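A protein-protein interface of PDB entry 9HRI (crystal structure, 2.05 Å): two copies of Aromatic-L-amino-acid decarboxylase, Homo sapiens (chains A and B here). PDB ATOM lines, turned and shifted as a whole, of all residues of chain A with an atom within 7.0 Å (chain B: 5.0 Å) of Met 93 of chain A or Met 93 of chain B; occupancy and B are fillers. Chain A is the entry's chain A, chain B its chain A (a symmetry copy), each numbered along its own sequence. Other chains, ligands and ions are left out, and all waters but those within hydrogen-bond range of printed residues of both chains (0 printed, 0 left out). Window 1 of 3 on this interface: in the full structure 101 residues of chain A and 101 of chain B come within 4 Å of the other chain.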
ATOM      1  N   PHE A   6       5.806 -19.843  12.119  1.00  0.00           N
ATOM      2  CA  PHE A   6       6.617 -19.401  10.988  1.00  0.00           C
ATOM      3  C   PHE A   6       7.998 -18.949  11.437  1.00  0.00           C
ATOM      4  O   PHE A   6       8.976 -19.125  10.700  1.00  0.00           O
ATOM      5  CB  PHE A   6       5.920 -18.269  10.229  1.00  0.00           C
ATOM      6  CG  PHE A   6       6.730 -17.723   9.085  1.00  0.00           C
ATOM      7  CD1 PHE A   6       7.016 -18.512   7.982  1.00  0.00           C
ATOM      8  CD2 PHE A   6       7.221 -16.429   9.123  1.00  0.00           C
ATOM      9  CE1 PHE A   6       7.766 -18.012   6.929  1.00  0.00           C
ATOM     10  CE2 PHE A   6       7.973 -15.924   8.077  1.00  0.00           C
ATOM     11  CZ  PHE A   6       8.245 -16.716   6.977  1.00  0.00           C
ATOM     12  N   ARG A   9       9.785 -22.417  11.625  1.00  0.00           N
ATOM     13  CA  ARG A   9       9.929 -23.096  10.341  1.00  0.00           C
ATOM     14  C   ARG A   9      10.610 -22.213   9.301  1.00  0.00           C
ATOM     15  O   ARG A   9      11.330 -22.726   8.436  1.00  0.00           O
ATOM     16  CB  ARG A   9       8.560 -23.557   9.841  1.00  0.00           C
ATOM     17  CG  ARG A   9       7.791 -24.403  10.849  1.00  0.00           C
ATOM     18  CD  ARG A   9       8.642 -25.549  11.367  1.00  0.00           C
ATOM     19  NE  ARG A   9       7.841 -26.586  12.007  1.00  0.00           N
ATOM     20  CZ  ARG A   9       8.302 -27.777  12.362  1.00  0.00           C
ATOM     21  NH1 ARG A   9       9.571 -28.107  12.184  1.00  0.00           N
ATOM     22  NH2 ARG A   9       7.472 -28.657  12.914  1.00  0.00           N
ATOM     23  N   GLY A  10      10.393 -20.897   9.365  1.00  0.00           N
ATOM     24  CA  GLY A  10      11.056 -20.000   8.430  1.00  0.00           C
ATOM     25  C   GLY A  10      12.566 -20.030   8.567  1.00  0.00           C
ATOM     26  O   GLY A  10      13.294 -20.103   7.573  1.00  0.00           O
ATOM     27  N   LYS A  11      13.059 -19.974   9.806  1.00  0.00           N
ATOM     28  CA  LYS A  11      14.499 -20.066  10.027  1.00  0.00           C
ATOM     29  C   LYS A  11      15.031 -21.453   9.692  1.00  0.00           C
ATOM     30  O   LYS A  11      16.175 -21.581   9.238  1.00  0.00           O
ATOM     31  CB  LYS A  11      14.837 -19.691  11.471  1.00  0.00           C
ATOM     32  CG  LYS A  11      14.350 -18.301  11.865  1.00  0.00           C
ATOM     33  CD  LYS A  11      14.815 -17.914  13.266  1.00  0.00           C
ATOM     34  CE  LYS A  11      14.249 -16.562  13.676  1.00  0.00           C
ATOM     35  NZ  LYS A  11      14.831 -16.071  14.959  1.00  0.00           N
ATOM     36  N   GLU A  12      14.228 -22.499   9.901  1.00  0.00           N
ATOM     37  CA  GLU A  12      14.649 -23.833   9.488  1.00  0.00           C
ATOM     38  C   GLU A  12      14.774 -23.920   7.972  1.00  0.00           C
ATOM     39  O   GLU A  12      15.701 -24.553   7.452  1.00  0.00           O
ATOM     40  CB  GLU A  12      13.667 -24.882  10.016  1.00  0.00           C
ATOM     41  CG  GLU A  12      13.710 -25.053  11.533  1.00  0.00           C
ATOM     42  CD  GLU A  12      12.671 -26.033  12.047  1.00  0.00           C
ATOM     43  OE1 GLU A  12      11.798 -26.448  11.255  1.00  0.00           O
ATOM     44  OE2 GLU A  12      12.725 -26.384  13.245  1.00  0.00           O
ATOM     45  N   MET A  13      13.854 -23.279   7.245  1.00  0.00           N
ATOM     46  CA  MET A  13      13.940 -23.283   5.790  1.00  0.00           C
ATOM     47  C   MET A  13      15.118 -22.453   5.294  1.00  0.00           C
ATOM     48  O   MET A  13      15.722 -22.795   4.271  1.00  0.00           O
ATOM     49  CB  MET A  13      12.634 -22.770   5.180  1.00  0.00           C
ATOM     50  CG  MET A  13      12.651 -22.694   3.661  1.00  0.00           C
ATOM     51  SD  MET A  13      12.744 -24.324   2.893  1.00  0.00           S
ATOM     52  CE  MET A  13      11.088 -24.925   3.206  1.00  0.00           C
ATOM     53  N   VAL A  14      15.457 -21.367   5.998  1.00  0.00           N
ATOM     54  CA  VAL A  14      16.653 -20.598   5.655  1.00  0.00           C
ATOM     55  C   VAL A  14      17.883 -21.494   5.716  1.00  0.00           C
ATOM     56  O   VAL A  14      18.721 -21.501   4.804  1.00  0.00           O
ATOM     57  CB  VAL A  14      16.801 -19.377   6.584  1.00  0.00           C
ATOM     58  CG1 VAL A  14      18.199 -18.791   6.462  1.00  0.00           C
ATOM     59  CG2 VAL A  14      15.764 -18.317   6.261  1.00  0.00           C
ATOM     60  N   ASP A  15      17.999 -22.280   6.789  1.00  0.00           N
ATOM     61  CA  ASP A  15      19.135 -23.185   6.932  1.00  0.00           C
ATOM     62  C   ASP A  15      19.123 -24.258   5.853  1.00  0.00           C
ATOM     63  O   ASP A  15      20.179 -24.625   5.324  1.00  0.00           O
ATOM     64  CB  ASP A  15      19.124 -23.827   8.318  1.00  0.00           C
ATOM     65  CG  ASP A  15      19.824 -22.980   9.353  1.00  0.00           C
ATOM     66  OD1 ASP A  15      20.708 -22.184   8.971  1.00  0.00           O
ATOM     67  OD2 ASP A  15      19.490 -23.112  10.549  1.00  0.00           O
ATOM     68  N   VAL A  17      17.834 -24.042   2.788  1.00  0.00           N
ATOM     69  CA  VAL A  17      18.236 -23.429   1.525  1.00  0.00           C
ATOM     70  C   VAL A  17      19.737 -23.173   1.511  1.00  0.00           C
ATOM     71  O   VAL A  17      20.418 -23.436   0.512  1.00  0.00           O
ATOM     72  CB  VAL A  17      17.435 -22.136   1.279  1.00  0.00           C
ATOM     73  CG1 VAL A  17      18.042 -21.339   0.135  1.00  0.00           C
ATOM     74  CG2 VAL A  17      15.978 -22.464   0.986  1.00  0.00           C
ATOM     75  N   TYR A  86      20.810 -14.010  -2.956  1.00  0.00           N
ATOM     76  CA  TYR A  86      20.190 -13.916  -1.641  1.00  0.00           C
ATOM     77  C   TYR A  86      19.510 -12.568  -1.397  1.00  0.00           C
ATOM     78  O   TYR A  86      18.463 -12.538  -0.736  1.00  0.00           O
ATOM     79  CB  TYR A  86      21.229 -14.202  -0.556  1.00  0.00           C
ATOM     80  CG  TYR A  86      21.810 -15.597  -0.655  1.00  0.00           C
ATOM     81  CD1 TYR A  86      20.984 -16.718  -0.630  1.00  0.00           C
ATOM     82  CD2 TYR A  86      23.178 -15.797  -0.789  1.00  0.00           C
ATOM     83  CE1 TYR A  86      21.509 -18.001  -0.727  1.00  0.00           C
ATOM     84  CE2 TYR A  86      23.710 -17.074  -0.889  1.00  0.00           C
ATOM     85  CZ  TYR A  86      22.875 -18.173  -0.858  1.00  0.00           C
ATOM     86  OH  TYR A  86      23.419 -19.442  -0.958  1.00  0.00           O
ATOM     87  N   ALA A  88      17.804 -10.828  -3.543  1.00  0.00           N
ATOM     88  CA  ALA A  88      16.496 -10.983  -4.171  1.00  0.00           C
ATOM     89  C   ALA A  88      15.614 -11.938  -3.376  1.00  0.00           C
ATOM     90  O   ALA A  88      14.406 -11.711  -3.246  1.00  0.00           O
ATOM     91  CB  ALA A  88      16.661 -11.472  -5.610  1.00  0.00           C
ATOM     92  N   MET A  89      16.202 -13.010  -2.838  1.00  0.00           N
ATOM     93  CA  MET A  89      15.443 -13.941  -2.007  1.00  0.00           C
ATOM     94  C   MET A  89      14.897 -13.257  -0.758  1.00  0.00           C
ATOM     95  O   MET A  89      13.752 -13.500  -0.363  1.00  0.00           O
ATOM     96  CB  MET A  89      16.323 -15.134  -1.631  1.00  0.00           C
ATOM     97  CG  MET A  89      16.745 -15.989  -2.820  1.00  0.00           C
ATOM     98  SD  MET A  89      17.586 -17.514  -2.335  1.00  0.00           S
ATOM     99  CE  MET A  89      16.377 -18.268  -1.249  1.00  0.00           C
ATOM    100  N   LEU A  90      15.701 -12.395  -0.126  1.00  0.00           N
ATOM    101  CA  LEU A  90      15.220 -11.668   1.047  1.00  0.00           C
ATOM    102  C   LEU A  90      14.063 -10.743   0.689  1.00  0.00           C
ATOM    103  O   LEU A  90      13.121 -10.584   1.473  1.00  0.00           O
ATOM    104  CB  LEU A  90      16.363 -10.870   1.680  1.00  0.00           C
ATOM    105  CG  LEU A  90      17.521 -11.669   2.282  1.00  0.00           C
ATOM    106  CD1 LEU A  90      18.747 -10.782   2.457  1.00  0.00           C
ATOM    107  CD2 LEU A  90      17.108 -12.272   3.613  1.00  0.00           C
ATOM    108  N   ALA A  91      14.115 -10.124  -0.491  1.00  0.00           N
ATOM    109  CA  ALA A  91      13.026  -9.245  -0.902  1.00  0.00           C
ATOM    110  C   ALA A  91      11.756 -10.037  -1.186  1.00  0.00           C
ATOM    111  O   ALA A  91      10.653  -9.595  -0.843  1.00  0.00           O
ATOM    112  CB  ALA A  91      13.439  -8.431  -2.128  1.00  0.00           C
ATOM    113  N   ASP A  92      11.892 -11.210  -1.810  1.00  0.00           N
ATOM    114  CA  ASP A  92      10.722 -12.037  -2.088  1.00  0.00           C
ATOM    115  C   ASP A  92      10.000 -12.438  -0.810  1.00  0.00           C
ATOM    116  O   ASP A  92       8.771 -12.568  -0.806  1.00  0.00           O
ATOM    117  CB  ASP A  92      11.128 -13.283  -2.879  1.00  0.00           C
ATOM    118  CG  ASP A  92      11.082 -13.061  -4.376  1.00  0.00           C
ATOM    119  OD1 ASP A  92      10.234 -12.258  -4.814  1.00  0.00           O
ATOM    120  OD2 ASP A  92      11.888 -13.676  -5.112  1.00  0.00           O
ATOM    121  N   MET A  93      10.742 -12.645   0.282  1.00  0.00           N
ATOM    122  CA  MET A  93      10.101 -12.986   1.547  1.00  0.00           C
ATOM    123  C   MET A  93       9.219 -11.841   2.021  1.00  0.00           C
ATOM    124  O   MET A  93       8.103 -12.061   2.510  1.00  0.00           O
ATOM    125  CB  MET A  93      11.157 -13.319   2.603  1.00  0.00           C
ATOM    126  CG  MET A  93      11.947 -14.592   2.305  1.00  0.00           C
ATOM    127  SD  MET A  93      13.375 -14.855   3.377  1.00  0.00           S
ATOM    128  CE  MET A  93      12.609 -14.640   4.972  1.00  0.00           C
ATOM    129  N   LEU A  94       9.705 -10.606   1.883  1.00  0.00           N
ATOM    130  CA  LEU A  94       8.902  -9.449   2.252  1.00  0.00           C
ATOM    131  C   LEU A  94       7.717  -9.271   1.314  1.00  0.00           C
ATOM    132  O   LEU A  94       6.647  -8.835   1.749  1.00  0.00           O
ATOM    133  CB  LEU A  94       9.768  -8.191   2.262  1.00  0.00           C
ATOM    134  CG  LEU A  94       9.157  -6.949   2.915  1.00  0.00           C
ATOM    135  CD1 LEU A  94       8.676  -7.242   4.329  1.00  0.00           C
ATOM    136  CD2 LEU A  94      10.173  -5.820   2.923  1.00  0.00           C
ATOM    137  N   CYS A  95       7.888  -9.609   0.031  1.00  0.00           N
ATOM    138  CA  CYS A  95       6.793  -9.472  -0.925  1.00  0.00           C
ATOM    139  C   CYS A  95       5.611 -10.355  -0.558  1.00  0.00           C
ATOM    140  O   CYS A  95       4.459  -9.981  -0.805  1.00  0.00           O
ATOM    141  CB  CYS A  95       7.274  -9.806  -2.337  1.00  0.00           C
ATOM    142  SG  CYS A  95       8.364  -8.571  -3.064  1.00  0.00           S
ATOM    143  N   GLY A  96       5.868 -11.526   0.026  1.00  0.00           N
ATOM    144  CA  GLY A  96       4.783 -12.384   0.465  1.00  0.00           C
ATOM    145  C   GLY A  96       3.939 -11.781   1.567  1.00  0.00           C
ATOM    146  O   GLY A  96       2.820 -12.246   1.802  1.00  0.00           O
ATOM    147  N   ALA A  97       4.446 -10.753   2.246  1.00  0.00           N
ATOM    148  CA  ALA A  97       3.712 -10.100   3.321  1.00  0.00           C
ATOM    149  C   ALA A  97       3.144  -8.741   2.934  1.00  0.00           C
ATOM    150  O   ALA A  97       2.070  -8.375   3.423  1.00  0.00           O
ATOM    151  CB  ALA A  97       4.613  -9.935   4.550  1.00  0.00           C
ATOM    152  N   ILE A  98       3.828  -7.982   2.081  1.00  0.00           N
ATOM    153  CA  ILE A  98       3.393  -6.635   1.726  1.00  0.00           C
ATOM    154  C   ILE A  98       3.098  -6.471   0.243  1.00  0.00           C
ATOM    155  O   ILE A  98       2.573  -5.421  -0.152  1.00  0.00           O
ATOM    156  CB  ILE A  98       4.418  -5.574   2.181  1.00  0.00           C
ATOM    157  CG1 ILE A  98       5.682  -5.650   1.323  1.00  0.00           C
ATOM    158  CG2 ILE A  98       4.756  -5.757   3.656  1.00  0.00           C
ATOM    159  CD1 ILE A  98       6.622  -4.485   1.526  1.00  0.00           C
ATOM    160  N   LEU A 360      10.953  -4.431  -5.474  1.00  0.00           N
ATOM    161  CA  LEU A 360      11.649  -4.650  -4.212  1.00  0.00           C
ATOM    162  C   LEU A 360      12.874  -5.534  -4.408  1.00  0.00           C
ATOM    163  O   LEU A 360      13.926  -5.286  -3.808  1.00  0.00           O
ATOM    164  CB  LEU A 360      10.698  -5.271  -3.185  1.00  0.00           C
ATOM    165  CG  LEU A 360      11.004  -4.978  -1.710  1.00  0.00           C
ATOM    166  CD1 LEU A 360      10.814  -3.498  -1.401  1.00  0.00           C
ATOM    167  CD2 LEU A 360      10.162  -5.845  -0.777  1.00  0.00           C
ATOM    168  N   GLY B  10      18.725 -14.117   6.451  1.00  0.00           N
ATOM    169  CA  GLY B  10      17.480 -14.820   6.175  1.00  0.00           C
ATOM    170  C   GLY B  10      16.634 -15.011   7.419  1.00  0.00           C
ATOM    171  O   GLY B  10      15.422 -14.776   7.407  1.00  0.00           O
ATOM    172  N   MET B  13      15.208 -11.716   8.455  1.00  0.00           N
ATOM    173  CA  MET B  13      14.041 -11.351   7.660  1.00  0.00           C
ATOM    174  C   MET B  13      12.815 -12.165   8.056  1.00  0.00           C
ATOM    175  O   MET B  13      11.692 -11.649   8.001  1.00  0.00           O
ATOM    176  CB  MET B  13      14.338 -11.527   6.169  1.00  0.00           C
ATOM    177  CG  MET B  13      13.157 -11.213   5.265  1.00  0.00           C
ATOM    178  SD  MET B  13      12.710  -9.464   5.301  1.00  0.00           S
ATOM    179  CE  MET B  13      14.071  -8.764   4.372  1.00  0.00           C
ATOM    180  N   VAL B  14      13.005 -13.428   8.452  1.00  0.00           N
ATOM    181  CA  VAL B  14      11.892 -14.224   8.968  1.00  0.00           C
ATOM    182  C   VAL B  14      11.270 -13.532  10.175  1.00  0.00           C
ATOM    183  O   VAL B  14      10.045 -13.395  10.277  1.00  0.00           O
ATOM    184  CB  VAL B  14      12.359 -15.651   9.319  1.00  0.00           C
ATOM    185  CG1 VAL B  14      11.309 -16.353  10.165  1.00  0.00           C
ATOM    186  CG2 VAL B  14      12.637 -16.457   8.062  1.00  0.00           C
ATOM    187  N   VAL B  17       9.376 -10.334   9.057  1.00  0.00           N
ATOM    188  CA  VAL B  17       8.080 -10.648   8.461  1.00  0.00           C
ATOM    189  C   VAL B  17       7.089 -11.074   9.536  1.00  0.00           C
ATOM    190  O   VAL B  17       5.927 -10.651   9.532  1.00  0.00           O
ATOM    191  CB  VAL B  17       8.241 -11.726   7.373  1.00  0.00           C
ATOM    192  CG1 VAL B  17       6.882 -12.272   6.956  1.00  0.00           C
ATOM    193  CG2 VAL B  17       8.977 -11.156   6.170  1.00  0.00           C
ATOM    194  N   MET B  89       4.749 -19.270   1.658  1.00  0.00           N
ATOM    195  CA  MET B  89       5.979 -18.497   1.808  1.00  0.00           C
ATOM    196  C   MET B  89       7.194 -19.406   1.954  1.00  0.00           C
ATOM    197  O   MET B  89       8.252 -19.133   1.374  1.00  0.00           O
ATOM    198  CB  MET B  89       5.856 -17.557   3.009  1.00  0.00           C
ATOM    199  CG  MET B  89       4.785 -16.485   2.848  1.00  0.00           C
ATOM    200  SD  MET B  89       4.812 -15.251   4.168  1.00  0.00           S
ATOM    201  CE  MET B  89       6.500 -14.657   4.078  1.00  0.00           C
ATOM    202  N   LEU B  90       7.064 -20.493   2.722  1.00  0.00           N
ATOM    203  CA  LEU B  90       8.175 -21.431   2.862  1.00  0.00           C
ATOM    204  C   LEU B  90       8.520 -22.083   1.529  1.00  0.00           C
ATOM    205  O   LEU B  90       9.696 -22.322   1.231  1.00  0.00           O
ATOM    206  CB  LEU B  90       7.838 -22.498   3.906  1.00  0.00           C
ATOM    207  CG  LEU B  90       7.665 -22.030   5.352  1.00  0.00           C
ATOM    208  CD1 LEU B  90       6.914 -23.075   6.165  1.00  0.00           C
ATOM    209  CD2 LEU B  90       9.018 -21.740   5.977  1.00  0.00           C
ATOM    210  N   ALA B  91       7.509 -22.382   0.712  1.00  0.00           N
ATOM    211  CA  ALA B  91       7.775 -22.985  -0.589  1.00  0.00           C
ATOM    212  C   ALA B  91       8.458 -21.997  -1.525  1.00  0.00           C
ATOM    213  O   ALA B  91       9.364 -22.373  -2.279  1.00  0.00           O
ATOM    214  CB  ALA B  91       6.476 -23.503  -1.207  1.00  0.00           C
ATOM    215  N   ASP B  92       8.039 -20.730  -1.490  1.00  0.00           N
ATOM    216  CA  ASP B  92       8.669 -19.721  -2.337  1.00  0.00           C
ATOM    217  C   ASP B  92      10.152 -19.575  -2.030  1.00  0.00           C
ATOM    218  O   ASP B  92      10.949 -19.301  -2.935  1.00  0.00           O
ATOM    219  CB  ASP B  92       7.961 -18.375  -2.176  1.00  0.00           C
ATOM    220  CG  ASP B  92       6.818 -18.199  -3.153  1.00  0.00           C
ATOM    221  OD1 ASP B  92       6.920 -18.751  -4.266  1.00  0.00           O
ATOM    222  OD2 ASP B  92       5.821 -17.519  -2.814  1.00  0.00           O
ATOM    223  N   MET B  93      10.543 -19.747  -0.766  1.00  0.00           N
ATOM    224  CA  MET B  93      11.958 -19.665  -0.420  1.00  0.00           C
ATOM    225  C   MET B  93      12.738 -20.776  -1.108  1.00  0.00           C
ATOM    226  O   MET B  93      13.844 -20.553  -1.615  1.00  0.00           O
ATOM    227  CB  MET B  93      12.138 -19.746   1.098  1.00  0.00           C
ATOM    228  CG  MET B  93      11.568 -18.547   1.851  1.00  0.00           C
ATOM    229  SD  MET B  93      11.517 -18.745   3.645  1.00  0.00           S
ATOM    230  CE  MET B  93      13.194 -19.264   3.947  1.00  0.00           C
ATOM    231  N   LEU B  94      12.173 -21.985  -1.133  1.00  0.00           N
ATOM    232  CA  LEU B  94      12.821 -23.090  -1.826  1.00  0.00           C
ATOM    233  C   LEU B  94      12.830 -22.874  -3.332  1.00  0.00           C
ATOM    234  O   LEU B  94      13.786 -23.272  -4.005  1.00  0.00           O
ATOM    235  CB  LEU B  94      12.126 -24.406  -1.480  1.00  0.00           C
ATOM    236  CG  LEU B  94      12.858 -25.688  -1.878  1.00  0.00           C
ATOM    237  CD1 LEU B  94      14.280 -25.710  -1.335  1.00  0.00           C
ATOM    238  CD2 LEU B  94      12.084 -26.897  -1.386  1.00  0.00           C
ATOM    239  N   CYS B  95      11.783 -22.243  -3.874  1.00  0.00           N
ATOM    240  CA  CYS B  95      11.727 -21.995  -5.311  1.00  0.00           C
ATOM    241  C   CYS B  95      12.865 -21.097  -5.772  1.00  0.00           C
ATOM    242  O   CYS B  95      13.359 -21.251  -6.895  1.00  0.00           O
ATOM    243  CB  CYS B  95      10.385 -21.373  -5.693  1.00  0.00           C
ATOM    244  SG  CYS B  95       8.988 -22.505  -5.605  1.00  0.00           S
ATOM    245  N   GLY B  96      13.293 -20.155  -4.929  1.00  0.00           N
ATOM    246  CA  GLY B  96      14.421 -19.312  -5.281  1.00  0.00           C
ATOM    247  C   GLY B  96      15.723 -20.068  -5.428  1.00  0.00           C
ATOM    248  O   GLY B  96      16.668 -19.545  -6.027  1.00  0.00           O
ATOM    249  N   ALA B  97      15.794 -21.290  -4.904  1.00  0.00           N
ATOM    250  CA  ALA B  97      17.000 -22.101  -4.995  1.00  0.00           C
ATOM    251  C   ALA B  97      16.897 -23.235  -6.007  1.00  0.00           C
ATOM    252  O   ALA B  97      17.905 -23.579  -6.633  1.00  0.00           O
ATOM    253  CB  ALA B  97      17.350 -22.685  -3.622  1.00  0.00           C
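CE of Met 89 of chain B touches CZ of Phe 6 of chain A, 3.96 Å away. Lys 11 of chain A touches Val 14 of chain B (N to CG2, 3.9 Å). Met 13 of chain A touches Met 93 of chain B (CG to CE, 3.5 Å). CG2 of Val 14 of chain A touches C of Gly 10 of chain B, at 3.6 Å. Met 93 of chain B touches Val 17 of chain A (O to CG2, 3.9 Å). Met 93 of chain B touches Met 89 of chain A (O to CE, 3.4 Å). Leu 90 of chain A touches Met 13 of chain B (O to CE, 3.6 Å). CG of Met 13 of chain B touches CE of Met 93 of chain A, at 3.5 Å. Met 93 of chain A touches Met 89 of chain B. Met 93 of chain A touches Met 93 of chain B.
Hydrophobic or aromatic side chains of chain B that line the printed part of chain A: Met 13, Val 14, Val 17, Met 89, Leu 90 and Met 93. Of the 22 printed residues of chain A, 10 touch a printed residue of chain B. Among the printed residues, 22 pairs touch across the chains. Among the printed residues, no Asp or Glu carboxylate lies within 4 Å of a Lys or Arg side-chain nitrogen of the other chain.
Of the printed residues of chain B, Gly 10 of chain A touches Val 14, Leu 90 and Met 93. Glu 12 of chain A touches none of the printed residues of chain B. Tyr 86 of chain A touches none of the printed residues of chain B. Printed residues of chain B within 4 Å of Met 93 of chain A: Gly 10 (3.7 Å), Met 13 (3.5 Å), Val 14 (3.6 Å), Val 17 (3.9 Å), Met 89 (3.4 Å) and Met 93 (3.999 Å). Of the printed residues of chain A, Met 89 of chain B touches Phe 6 (3.96 Å) and Met 93 (3.4 Å). Of the printed residues of chain A, Met 93 of chain B touches Gly 10 (3.7 Å), Met 13 (3.5 Å), Val 14 (3.6 Å), Val 17 (3.9 Å), Met 89 (3.4 Å) and Met 93 (3.999 Å). The nearest printed residue of chain B that does not touch Met 93 of chain A is Asp 92 of chain B (6.8 Å). The nearest printed residue of chain A that does not touch Met 93 of chain B is Phe 6 of chain A (5.0 Å).
The guanidinium group (NH1) of Arg 9 of chain A lies within salt-bridge range of the side-chain carboxylate (OE1) of Glu 12 of chain A, at 2.9 Å.
Gly 10 of chain A touches Val 14 of chain B, and with the chains exchanged Val 14 of chain A touches Gly 10 of chain B. Gly 10 of chain A touches Met 93 of chain B, and with the chains exchanged Met 93 of chain A touches Gly 10 of chain B. Met 13 of chain A touches Met 93 of chain B, and with the chains exchanged Met 93 of chain A touches Met 13 of chain B. Val 14 of chain A touches Met 93 of chain B, and with the chains exchanged Met 93 of chain A touches Val 14 of chain B. Positions printed for both chains: 10, 13, 14, 17, 89, 90, 91, 92, 93, 94, 95, 96 and 97. Of the 22 pairs that touch across the chains among the printed residues, 17 have their exchanged pair printed and touching as well.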
